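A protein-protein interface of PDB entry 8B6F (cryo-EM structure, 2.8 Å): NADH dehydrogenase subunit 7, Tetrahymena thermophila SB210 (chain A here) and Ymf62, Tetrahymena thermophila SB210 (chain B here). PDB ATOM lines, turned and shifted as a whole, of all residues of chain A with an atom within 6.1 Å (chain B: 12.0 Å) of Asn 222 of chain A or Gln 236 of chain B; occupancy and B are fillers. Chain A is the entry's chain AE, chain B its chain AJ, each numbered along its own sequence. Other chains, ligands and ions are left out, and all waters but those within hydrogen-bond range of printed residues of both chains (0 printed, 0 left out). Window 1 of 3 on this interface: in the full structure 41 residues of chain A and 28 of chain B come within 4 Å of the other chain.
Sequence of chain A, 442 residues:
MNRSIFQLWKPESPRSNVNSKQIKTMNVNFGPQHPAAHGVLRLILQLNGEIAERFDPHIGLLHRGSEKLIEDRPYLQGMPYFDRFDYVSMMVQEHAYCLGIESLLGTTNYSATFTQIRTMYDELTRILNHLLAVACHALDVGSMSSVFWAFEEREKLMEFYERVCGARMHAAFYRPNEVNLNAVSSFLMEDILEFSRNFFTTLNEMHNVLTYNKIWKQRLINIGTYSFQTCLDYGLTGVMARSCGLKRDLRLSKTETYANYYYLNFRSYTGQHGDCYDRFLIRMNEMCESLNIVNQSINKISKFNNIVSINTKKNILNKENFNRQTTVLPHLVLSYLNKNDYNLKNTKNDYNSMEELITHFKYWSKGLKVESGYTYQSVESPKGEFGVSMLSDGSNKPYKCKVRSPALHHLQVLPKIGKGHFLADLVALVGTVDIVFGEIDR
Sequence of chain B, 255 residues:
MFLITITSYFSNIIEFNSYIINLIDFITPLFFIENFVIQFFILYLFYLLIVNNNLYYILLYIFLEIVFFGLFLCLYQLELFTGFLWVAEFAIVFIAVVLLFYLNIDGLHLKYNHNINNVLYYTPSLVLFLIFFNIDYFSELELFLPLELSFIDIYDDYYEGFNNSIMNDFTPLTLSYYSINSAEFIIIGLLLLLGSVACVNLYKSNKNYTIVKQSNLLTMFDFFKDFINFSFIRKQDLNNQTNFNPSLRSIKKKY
The side-chain amino group (NZ) of Lys 217 of chain A lies within hydrogen-bond range of the backbone carbonyl oxygen (O) of Thr 242 of chain B (2.7 Å). The backbone carbonyl oxygen of Phe 244 of chain B lies within hydrogen-bond range of the side-chain amino group of Lys 217 of chain A (3.4 Å). The side-chain amide oxygen (OE1) of Gln 241 of chain B lies close to the backbone carbonyl oxygen (O) of Gln 218 of chain A (3.4 Å). The backbone carbonyl oxygen (O) of Ile 221 of chain A lies within hydrogen-bond range of the side-chain amide nitrogen (NE2) of Gln 241 of chain B, 2.7 Å away. NH1 of Arg 234 of chain B is in hydrogen-bond range of NE2 of His 421 of chain A, 3.2 Å away.
The backbone NH (N) of Asn 222 of chain A sits at hydrogen-bond distance from the side-chain carboxylate (OD2) of Asp 275 of chain A. O of Ile 223 of chain A is in hydrogen-bond range of N of Cys 276 of chain A (3.1 Å). The backbone NH of Gly 224 of chain A sits at hydrogen-bond distance from a ring nitrogen (NE2) of His 421 of chain A, at 3.4 Å.
Of the printed residues of chain B, Lys 217 of chain A touches Gln 241 (3.7 Å), Thr 242 (2.7 Å) and Phe 244 (3.4 Å). Ile 221 of chain A touches just these residues of chain B: Gln 241 and Phe 244. Ile 223 of chain A touches one residue of chain B. Gly 224 of chain A touches none of the printed residues of chain B. No residue of chain B comes within 4 Å of Thr 225 of chain A. No residue of chain B comes within 4 Å of Asp 275 of chain A. No residue of chain B comes within 4 Å of Cys 276 of chain A. Of the printed residues of chain A, Gln 236 of chain B touches Asn 222 and His 421. Of the printed residues of chain A, Leu 238 of chain B touches Gln 218. Of the printed residues of chain A, Gln 241 of chain B touches Lys 217 (3.7 Å), Gln 218 (3.4 Å), Ile 221 (2.7 Å) and Ile 223 (3.8 Å). Printed residues of chain A within 4 Å of Thr 242 of chain B: Lys 217 (2.7 Å) and Gln 218 (3.9 Å). Of the printed residues of chain A, Pro 246 of chain B touches Tyr 277. The nearest residue of chain A that does not touch Gln 236 of chain B is Ile 223 of chain A (4.1 Å).
Hydrophobic or aromatic side chains of chain A within 4 Å of the printed part of chain B: Ile 221, Ile 223, Tyr 277 and His 421. Among the printed residues, 14 pairs touch across the chains.
Among the printed residues, pairs that only touch across the chains: Ile 221 of chain A with Phe 244 of chain B, Asn 222 of chain A with Gln 236 of chain B, His 421 of chain A with Gln 236 of chain B, Tyr 277 of chain A with Pro 246 of chain B, Lys 217 of chain A with Gln 241 of chain B, Gln 218 of chain A with Leu 238 of chain B, Ile 223 of chain A with Gln 241 of chain B, Tyr 277 of chain A with Phe 244 of chain B and Gln 218 of chain A with Thr 242 of chain B.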
ATOM      1  N   LYS A 217      20.294  26.854   0.724  1.00  0.00           N
ATOM      2  CA  LYS A 217      19.745  25.502   0.754  1.00  0.00           C
ATOM      3  C   LYS A 217      18.680  25.311  -0.318  1.00  0.00           C
ATOM      4  O   LYS A 217      18.625  24.260  -0.966  1.00  0.00           O
ATOM      5  CB  LYS A 217      19.180  25.195   2.140  1.00  0.00           C
ATOM      6  CG  LYS A 217      20.249  24.915   3.181  1.00  0.00           C
ATOM      7  CD  LYS A 217      19.664  24.294   4.438  1.00  0.00           C
ATOM      8  CE  LYS A 217      18.762  25.261   5.173  1.00  0.00           C
ATOM      9  NZ  LYS A 217      18.256  24.677   6.446  1.00  0.00           N
ATOM     10  N   GLN A 218      17.821  26.311  -0.517  1.00  0.00           N
ATOM     11  CA  GLN A 218      16.778  26.197  -1.531  1.00  0.00           C
ATOM     12  C   GLN A 218      17.352  26.285  -2.938  1.00  0.00           C
ATOM     13  O   GLN A 218      16.753  25.761  -3.883  1.00  0.00           O
ATOM     14  CB  GLN A 218      15.711  27.269  -1.317  1.00  0.00           C
ATOM     15  CG  GLN A 218      14.904  27.068  -0.047  1.00  0.00           C
ATOM     16  CD  GLN A 218      13.832  28.117   0.136  1.00  0.00           C
ATOM     17  OE1 GLN A 218      13.782  29.106  -0.591  1.00  0.00           O
ATOM     18  NE2 GLN A 218      12.961  27.903   1.114  1.00  0.00           N
ATOM     19  N   LEU A 220      20.481  25.048  -3.845  1.00  0.00           N
ATOM     20  CA  LEU A 220      21.288  23.877  -4.173  1.00  0.00           C
ATOM     21  C   LEU A 220      20.563  22.558  -3.922  1.00  0.00           C
ATOM     22  O   LEU A 220      20.611  21.666  -4.772  1.00  0.00           O
ATOM     23  CB  LEU A 220      22.597  23.907  -3.373  1.00  0.00           C
ATOM     24  CG  LEU A 220      23.554  25.075  -3.631  1.00  0.00           C
ATOM     25  CD1 LEU A 220      24.948  24.700  -3.175  1.00  0.00           C
ATOM     26  CD2 LEU A 220      23.574  25.515  -5.084  1.00  0.00           C
ATOM     27  N   ILE A 221      19.912  22.399  -2.767  1.00  0.00           N
ATOM     28  CA  ILE A 221      19.334  21.104  -2.421  1.00  0.00           C
ATOM     29  C   ILE A 221      18.404  20.641  -3.530  1.00  0.00           C
ATOM     30  O   ILE A 221      17.585  21.410  -4.044  1.00  0.00           O
ATOM     31  CB  ILE A 221      18.604  21.138  -1.067  1.00  0.00           C
ATOM     32  CG1 ILE A 221      19.598  21.340   0.072  1.00  0.00           C
ATOM     33  CG2 ILE A 221      17.811  19.854  -0.842  1.00  0.00           C
ATOM     34  CD1 ILE A 221      18.950  21.783   1.343  1.00  0.00           C
ATOM     35  N   ASN A 222      18.525  19.367  -3.894  1.00  0.00           N
ATOM     36  CA  ASN A 222      17.645  18.739  -4.876  1.00  0.00           C
ATOM     37  C   ASN A 222      17.763  19.369  -6.259  1.00  0.00           C
ATOM     38  O   ASN A 222      16.812  19.349  -7.042  1.00  0.00           O
ATOM     39  CB  ASN A 222      16.188  18.767  -4.417  1.00  0.00           C
ATOM     40  CG  ASN A 222      15.456  17.485  -4.750  1.00  0.00           C
ATOM     41  OD1 ASN A 222      15.224  17.179  -5.921  1.00  0.00           O
ATOM     42  ND2 ASN A 222      15.101  16.721  -3.728  1.00  0.00           N
ATOM     43  N   ILE A 223      18.929  19.918  -6.574  1.00  0.00           N
ATOM     44  CA  ILE A 223      19.219  20.432  -7.904  1.00  0.00           C
ATOM     45  C   ILE A 223      20.378  19.593  -8.410  1.00  0.00           C
ATOM     46  O   ILE A 223      21.370  19.404  -7.697  1.00  0.00           O
ATOM     47  CB  ILE A 223      19.551  21.940  -7.892  1.00  0.00           C
ATOM     48  CG1 ILE A 223      18.273  22.780  -7.912  1.00  0.00           C
ATOM     49  CG2 ILE A 223      20.414  22.335  -9.076  1.00  0.00           C
ATOM     50  CD1 ILE A 223      17.583  22.901  -6.588  1.00  0.00           C
ATOM     51  N   GLY A 224      20.248  19.091  -9.630  1.00  0.00           N
ATOM     52  CA  GLY A 224      21.304  18.304 -10.228  1.00  0.00           C
ATOM     53  C   GLY A 224      21.398  16.911  -9.647  1.00  0.00           C
ATOM     54  O   GLY A 224      22.442  16.270  -9.768  1.00  0.00           O
ATOM     55  N   THR A 225      20.332  16.428  -9.006  1.00  0.00           N
ATOM     56  CA  THR A 225      20.390  15.145  -8.317  1.00  0.00           C
ATOM     57  C   THR A 225      20.697  14.036  -9.314  1.00  0.00           C
ATOM     58  O   THR A 225      20.123  13.992 -10.404  1.00  0.00           O
ATOM     59  CB  THR A 225      19.060  14.859  -7.609  1.00  0.00           C
ATOM     60  OG1 THR A 225      18.899  15.750  -6.500  1.00  0.00           O
ATOM     61  CG2 THR A 225      19.005  13.423  -7.091  1.00  0.00           C
ATOM     62  N   ASP A 275      23.280  15.828  -5.009  1.00  0.00           N
ATOM     63  CA  ASP A 275      22.845  17.159  -5.408  1.00  0.00           C
ATOM     64  C   ASP A 275      23.937  18.186  -5.134  1.00  0.00           C
ATOM     65  O   ASP A 275      24.955  17.902  -4.501  1.00  0.00           O
ATOM     66  CB  ASP A 275      21.551  17.547  -4.683  1.00  0.00           C
ATOM     67  CG  ASP A 275      21.634  17.328  -3.191  1.00  0.00           C
ATOM     68  OD1 ASP A 275      22.732  16.989  -2.705  1.00  0.00           O
ATOM     69  OD2 ASP A 275      20.604  17.486  -2.504  1.00  0.00           O
ATOM     70  N   CYS A 276      23.698  19.401  -5.632  1.00  0.00           N
ATOM     71  CA  CYS A 276      24.682  20.474  -5.523  1.00  0.00           C
ATOM     72  C   CYS A 276      25.019  20.780  -4.071  1.00  0.00           C
ATOM     73  O   CYS A 276      26.164  21.114  -3.748  1.00  0.00           O
ATOM     74  CB  CYS A 276      24.163  21.733  -6.216  1.00  0.00           C
ATOM     75  SG  CYS A 276      23.967  21.578  -7.999  1.00  0.00           S
ATOM     76  N   TYR A 277      24.035  20.676  -3.178  1.00  0.00           N
ATOM     77  CA  TYR A 277      24.292  20.937  -1.767  1.00  0.00           C
ATOM     78  C   TYR A 277      25.284  19.932  -1.198  1.00  0.00           C
ATOM     79  O   TYR A 277      26.219  20.309  -0.483  1.00  0.00           O
ATOM     80  CB  TYR A 277      22.980  20.907  -0.986  1.00  0.00           C
ATOM     81  CG  TYR A 277      23.066  21.524   0.392  1.00  0.00           C
ATOM     82  CD1 TYR A 277      23.328  22.879   0.552  1.00  0.00           C
ATOM     83  CD2 TYR A 277      22.864  20.757   1.529  1.00  0.00           C
ATOM     84  CE1 TYR A 277      23.399  23.447   1.806  1.00  0.00           C
ATOM     85  CE2 TYR A 277      22.934  21.319   2.789  1.00  0.00           C
ATOM     86  CZ  TYR A 277      23.200  22.663   2.919  1.00  0.00           C
ATOM     87  OH  TYR A 277      23.268  23.226   4.170  1.00  0.00           O
ATOM     88  N   HIS A 421      15.797  22.020 -15.640  1.00  0.00           N
ATOM     89  CA  HIS A 421      16.019  23.099 -14.691  1.00  0.00           C
ATOM     90  C   HIS A 421      15.915  24.464 -15.366  1.00  0.00           C
ATOM     91  O   HIS A 421      15.972  24.590 -16.590  1.00  0.00           O
ATOM     92  CB  HIS A 421      17.392  22.948 -14.035  1.00  0.00           C
ATOM     93  CG  HIS A 421      17.436  21.901 -12.970  1.00  0.00           C
ATOM     94  ND1 HIS A 421      16.731  22.010 -11.790  1.00  0.00           N
ATOM     95  CD2 HIS A 421      18.108  20.728 -12.898  1.00  0.00           C
ATOM     96  CE1 HIS A 421      16.962  20.948 -11.041  1.00  0.00           C
ATOM     97  NE2 HIS A 421      17.795  20.154 -11.690  1.00  0.00           N
ATOM     98  N   ASP A 425      19.085  27.861 -12.278  1.00  0.00           N
ATOM     99  CA  ASP A 425      19.625  26.586 -11.824  1.00  0.00           C
ATOM    100  C   ASP A 425      20.759  26.096 -12.711  1.00  0.00           C
ATOM    101  O   ASP A 425      21.689  25.449 -12.218  1.00  0.00           O
ATOM    102  CB  ASP A 425      18.520  25.533 -11.779  1.00  0.00           C
ATOM    103  CG  ASP A 425      17.545  25.759 -10.646  1.00  0.00           C
ATOM    104  OD1 ASP A 425      17.956  26.324  -9.612  1.00  0.00           O
ATOM    105  OD2 ASP A 425      16.368  25.368 -10.787  1.00  0.00           O
ATOM    106  N   PHE B 232       9.954  18.580 -19.920  1.00  0.00           N
ATOM    107  CA  PHE B 232       9.516  18.428 -18.543  1.00  0.00           C
ATOM    108  C   PHE B 232      10.152  19.508 -17.682  1.00  0.00           C
ATOM    109  O   PHE B 232      11.146  20.131 -18.060  1.00  0.00           O
ATOM    110  CB  PHE B 232       9.857  17.038 -17.994  1.00  0.00           C
ATOM    111  CG  PHE B 232      11.329  16.783 -17.868  1.00  0.00           C
ATOM    112  CD1 PHE B 232      12.076  16.395 -18.967  1.00  0.00           C
ATOM    113  CD2 PHE B 232      11.964  16.922 -16.646  1.00  0.00           C
ATOM    114  CE1 PHE B 232      13.430  16.160 -18.852  1.00  0.00           C
ATOM    115  CE2 PHE B 232      13.319  16.689 -16.524  1.00  0.00           C
ATOM    116  CZ  PHE B 232      14.052  16.307 -17.629  1.00  0.00           C
ATOM    117  N   ILE B 233       9.552  19.725 -16.513  1.00  0.00           N
ATOM    118  CA  ILE B 233      10.025  20.691 -15.531  1.00  0.00           C
ATOM    119  C   ILE B 233      10.267  19.957 -14.220  1.00  0.00           C
ATOM    120  O   ILE B 233       9.460  19.115 -13.811  1.00  0.00           O
ATOM    121  CB  ILE B 233       9.020  21.843 -15.334  1.00  0.00           C
ATOM    122  CG1 ILE B 233       8.761  22.540 -16.671  1.00  0.00           C
ATOM    123  CG2 ILE B 233       9.537  22.836 -14.297  1.00  0.00           C
ATOM    124  CD1 ILE B 233       7.718  23.633 -16.611  1.00  0.00           C
ATOM    125  N   ARG B 234      11.382  20.271 -13.568  1.00  0.00           N
ATOM    126  CA  ARG B 234      11.755  19.625 -12.318  1.00  0.00           C
ATOM    127  C   ARG B 234      11.229  20.433 -11.140  1.00  0.00           C
ATOM    128  O   ARG B 234      11.388  21.657 -11.097  1.00  0.00           O
ATOM    129  CB  ARG B 234      13.273  19.472 -12.225  1.00  0.00           C
ATOM    130  CG  ARG B 234      13.864  18.686 -13.379  1.00  0.00           C
ATOM    131  CD  ARG B 234      15.345  18.431 -13.190  1.00  0.00           C
ATOM    132  NE  ARG B 234      15.888  17.633 -14.281  1.00  0.00           N
ATOM    133  CZ  ARG B 234      17.121  17.149 -14.317  1.00  0.00           C
ATOM    134  NH1 ARG B 234      17.977  17.363 -13.331  1.00  0.00           N
ATOM    135  NH2 ARG B 234      17.505  16.426 -15.364  1.00  0.00           N
ATOM    136  N   LYS B 235      10.607  19.744 -10.189  1.00  0.00           N
ATOM    137  CA  LYS B 235       9.982  20.367  -9.033  1.00  0.00           C
ATOM    138  C   LYS B 235      10.789  20.060  -7.780  1.00  0.00           C
ATOM    139  O   LYS B 235      11.357  18.973  -7.645  1.00  0.00           O
ATOM    140  CB  LYS B 235       8.542  19.868  -8.862  1.00  0.00           C
ATOM    141  CG  LYS B 235       7.831  20.408  -7.628  1.00  0.00           C
ATOM    142  CD  LYS B 235       6.463  19.765  -7.442  1.00  0.00           C
ATOM    143  CE  LYS B 235       5.488  20.204  -8.520  1.00  0.00           C
ATOM    144  NZ  LYS B 235       4.138  19.602  -8.326  1.00  0.00           N
ATOM    145  N   GLN B 236      10.839  21.027  -6.868  1.00  0.00           N
ATOM    146  CA  GLN B 236      11.461  20.849  -5.566  1.00  0.00           C
ATOM    147  C   GLN B 236      10.488  21.296  -4.486  1.00  0.00           C
ATOM    148  O   GLN B 236       9.693  22.218  -4.686  1.00  0.00           O
ATOM    149  CB  GLN B 236      12.775  21.636  -5.441  1.00  0.00           C
ATOM    150  CG  GLN B 236      13.836  21.256  -6.463  1.00  0.00           C
ATOM    151  CD  GLN B 236      13.753  22.076  -7.734  1.00  0.00           C
ATOM    152  OE1 GLN B 236      13.318  23.226  -7.719  1.00  0.00           O
ATOM    153  NE2 GLN B 236      14.178  21.486  -8.847  1.00  0.00           N
ATOM    154  N   ASP B 237      10.557  20.630  -3.338  1.00  0.00           N
ATOM    155  CA  ASP B 237       9.721  20.965  -2.190  1.00  0.00           C
ATOM    156  C   ASP B 237      10.474  21.976  -1.335  1.00  0.00           C
ATOM    157  O   ASP B 237      11.483  21.641  -0.708  1.00  0.00           O
ATOM    158  CB  ASP B 237       9.374  19.711  -1.392  1.00  0.00           C
ATOM    159  CG  ASP B 237       8.277  19.953  -0.374  1.00  0.00           C
ATOM    160  OD1 ASP B 237       7.101  20.052  -0.781  1.00  0.00           O
ATOM    161  OD2 ASP B 237       8.589  20.047   0.830  1.00  0.00           O
ATOM    162  N   LEU B 238       9.982  23.214  -1.310  1.00  0.00           N
ATOM    163  CA  LEU B 238      10.697  24.280  -0.618  1.00  0.00           C
ATOM    164  C   LEU B 238      10.746  24.035   0.885  1.00  0.00           C
ATOM    165  O   LEU B 238      11.754  24.332   1.533  1.00  0.00           O
ATOM    166  CB  LEU B 238      10.048  25.625  -0.932  1.00  0.00           C
ATOM    167  CG  LEU B 238       9.933  25.934  -2.429  1.00  0.00           C
ATOM    168  CD1 LEU B 238       9.262  27.268  -2.648  1.00  0.00           C
ATOM    169  CD2 LEU B 238      11.297  25.918  -3.104  1.00  0.00           C
ATOM    170  N   ASN B 239       9.669  23.497   1.458  1.00  0.00           N
ATOM    171  CA  ASN B 239       9.667  23.198   2.887  1.00  0.00           C
ATOM    172  C   ASN B 239      10.747  22.180   3.228  1.00  0.00           C
ATOM    173  O   ASN B 239      11.475  22.334   4.215  1.00  0.00           O
ATOM    174  CB  ASN B 239       8.292  22.693   3.317  1.00  0.00           C
ATOM    175  CG  ASN B 239       7.202  23.715   3.080  1.00  0.00           C
ATOM    176  OD1 ASN B 239       6.273  23.481   2.307  1.00  0.00           O
ATOM    177  ND2 ASN B 239       7.308  24.857   3.748  1.00  0.00           N
ATOM    178  N   ASN B 240      10.854  21.117   2.430  1.00  0.00           N
ATOM    179  CA  ASN B 240      11.895  20.125   2.666  1.00  0.00           C
ATOM    180  C   ASN B 240      13.279  20.726   2.471  1.00  0.00           C
ATOM    181  O   ASN B 240      14.212  20.414   3.220  1.00  0.00           O
ATOM    182  CB  ASN B 240      11.695  18.924   1.742  1.00  0.00           C
ATOM    183  CG  ASN B 240      10.444  18.139   2.072  1.00  0.00           C
ATOM    184  OD1 ASN B 240      10.029  18.067   3.229  1.00  0.00           O
ATOM    185  ND2 ASN B 240       9.832  17.545   1.055  1.00  0.00           N
ATOM    186  N   GLN B 241      13.436  21.589   1.465  1.00  0.00           N
ATOM    187  CA  GLN B 241      14.728  22.229   1.238  1.00  0.00           C
ATOM    188  C   GLN B 241      15.150  23.070   2.435  1.00  0.00           C
ATOM    189  O   GLN B 241      16.316  23.038   2.844  1.00  0.00           O
ATOM    190  CB  GLN B 241      14.673  23.092  -0.023  1.00  0.00           C
ATOM    191  CG  GLN B 241      14.647  22.301  -1.315  1.00  0.00           C
ATOM    192  CD  GLN B 241      14.615  23.197  -2.533  1.00  0.00           C
ATOM    193  OE1 GLN B 241      14.061  24.293  -2.496  1.00  0.00           O
ATOM    194  NE2 GLN B 241      15.220  22.739  -3.622  1.00  0.00           N
ATOM    195  N   THR B 242      14.220  23.836   3.010  1.00  0.00           N
ATOM    196  CA  THR B 242      14.575  24.701   4.131  1.00  0.00           C
ATOM    197  C   THR B 242      14.770  23.911   5.419  1.00  0.00           C
ATOM    198  O   THR B 242      15.573  24.310   6.269  1.00  0.00           O
ATOM    199  CB  THR B 242      13.512  25.786   4.331  1.00  0.00           C
ATOM    200  OG1 THR B 242      13.900  26.648   5.407  1.00  0.00           O
ATOM    201  CG2 THR B 242      12.158  25.180   4.647  1.00  0.00           C
ATOM    202  N   ASN B 243      14.054  22.803   5.588  1.00  0.00           N
ATOM    203  CA  ASN B 243      14.174  21.982   6.785  1.00  0.00           C
ATOM    204  C   ASN B 243      15.282  20.942   6.686  1.00  0.00           C
ATOM    205  O   ASN B 243      15.545  20.246   7.671  1.00  0.00           O
ATOM    206  CB  ASN B 243      12.844  21.278   7.072  1.00  0.00           C
ATOM    207  CG  ASN B 243      11.714  22.253   7.332  1.00  0.00           C
ATOM    208  OD1 ASN B 243      11.933  23.351   7.840  1.00  0.00           O
ATOM    209  ND2 ASN B 243      10.496  21.853   6.986  1.00  0.00           N
ATOM    210  N   PHE B 244      15.933  20.822   5.534  1.00  0.00           N
ATOM    211  CA  PHE B 244      16.997  19.843   5.369  1.00  0.00           C
ATOM    212  C   PHE B 244      18.137  20.121   6.341  1.00  0.00           C
ATOM    213  O   PHE B 244      18.500  21.274   6.587  1.00  0.00           O
ATOM    214  CB  PHE B 244      17.508  19.876   3.928  1.00  0.00           C
ATOM    215  CG  PHE B 244      18.532  18.827   3.619  1.00  0.00           C
ATOM    216  CD1 PHE B 244      18.146  17.566   3.198  1.00  0.00           C
ATOM    217  CD2 PHE B 244      19.882  19.109   3.727  1.00  0.00           C
ATOM    218  CE1 PHE B 244      19.087  16.601   2.906  1.00  0.00           C
ATOM    219  CE2 PHE B 244      20.829  18.149   3.437  1.00  0.00           C
ATOM    220  CZ  PHE B 244      20.431  16.893   3.024  1.00  0.00           C
ATOM    221  N   ASN B 245      18.704  19.049   6.899  1.00  0.00           N
ATOM    222  CA  ASN B 245      19.823  19.152   7.825  1.00  0.00           C
ATOM    223  C   ASN B 245      21.096  18.681   7.139  1.00  0.00           C
ATOM    224  O   ASN B 245      21.193  17.493   6.796  1.00  0.00           O
ATOM    225  CB  ASN B 245      19.561  18.323   9.080  1.00  0.00           C
ATOM    226  CG  ASN B 245      18.370  18.824   9.869  1.00  0.00           C
ATOM    227  OD1 ASN B 245      18.473  19.792  10.623  1.00  0.00           O
ATOM    228  ND2 ASN B 245      17.231  18.163   9.704  1.00  0.00           N
ATOM    229  N   PRO B 246      22.090  19.541   6.920  1.00  0.00           N
ATOM    230  CA  PRO B 246      23.303  19.095   6.223  1.00  0.00           C
ATOM    231  C   PRO B 246      24.021  17.988   6.982  1.00  0.00           C
ATOM    232  O   PRO B 246      24.006  17.933   8.212  1.00  0.00           O
ATOM    233  CB  PRO B 246      24.158  20.366   6.143  1.00  0.00           C
ATOM    234  CG  PRO B 246      23.624  21.261   7.195  1.00  0.00           C
ATOM    235  CD  PRO B 246      22.170  20.962   7.302  1.00  0.00           C
ATOM    236  N   SER B 247      24.652  17.096   6.223  1.00  0.00           N
ATOM    237  CA  SER B 247      25.378  15.975   6.802  1.00  0.00           C
ATOM    238  C   SER B 247      26.173  15.279   5.707  1.00  0.00           C
ATOM    239  O   SER B 247      25.780  15.293   4.537  1.00  0.00           O
ATOM    240  CB  SER B 247      24.423  14.982   7.475  1.00  0.00           C
ATOM    241  OG  SER B 247      25.121  13.847   7.953  1.00  0.00           O
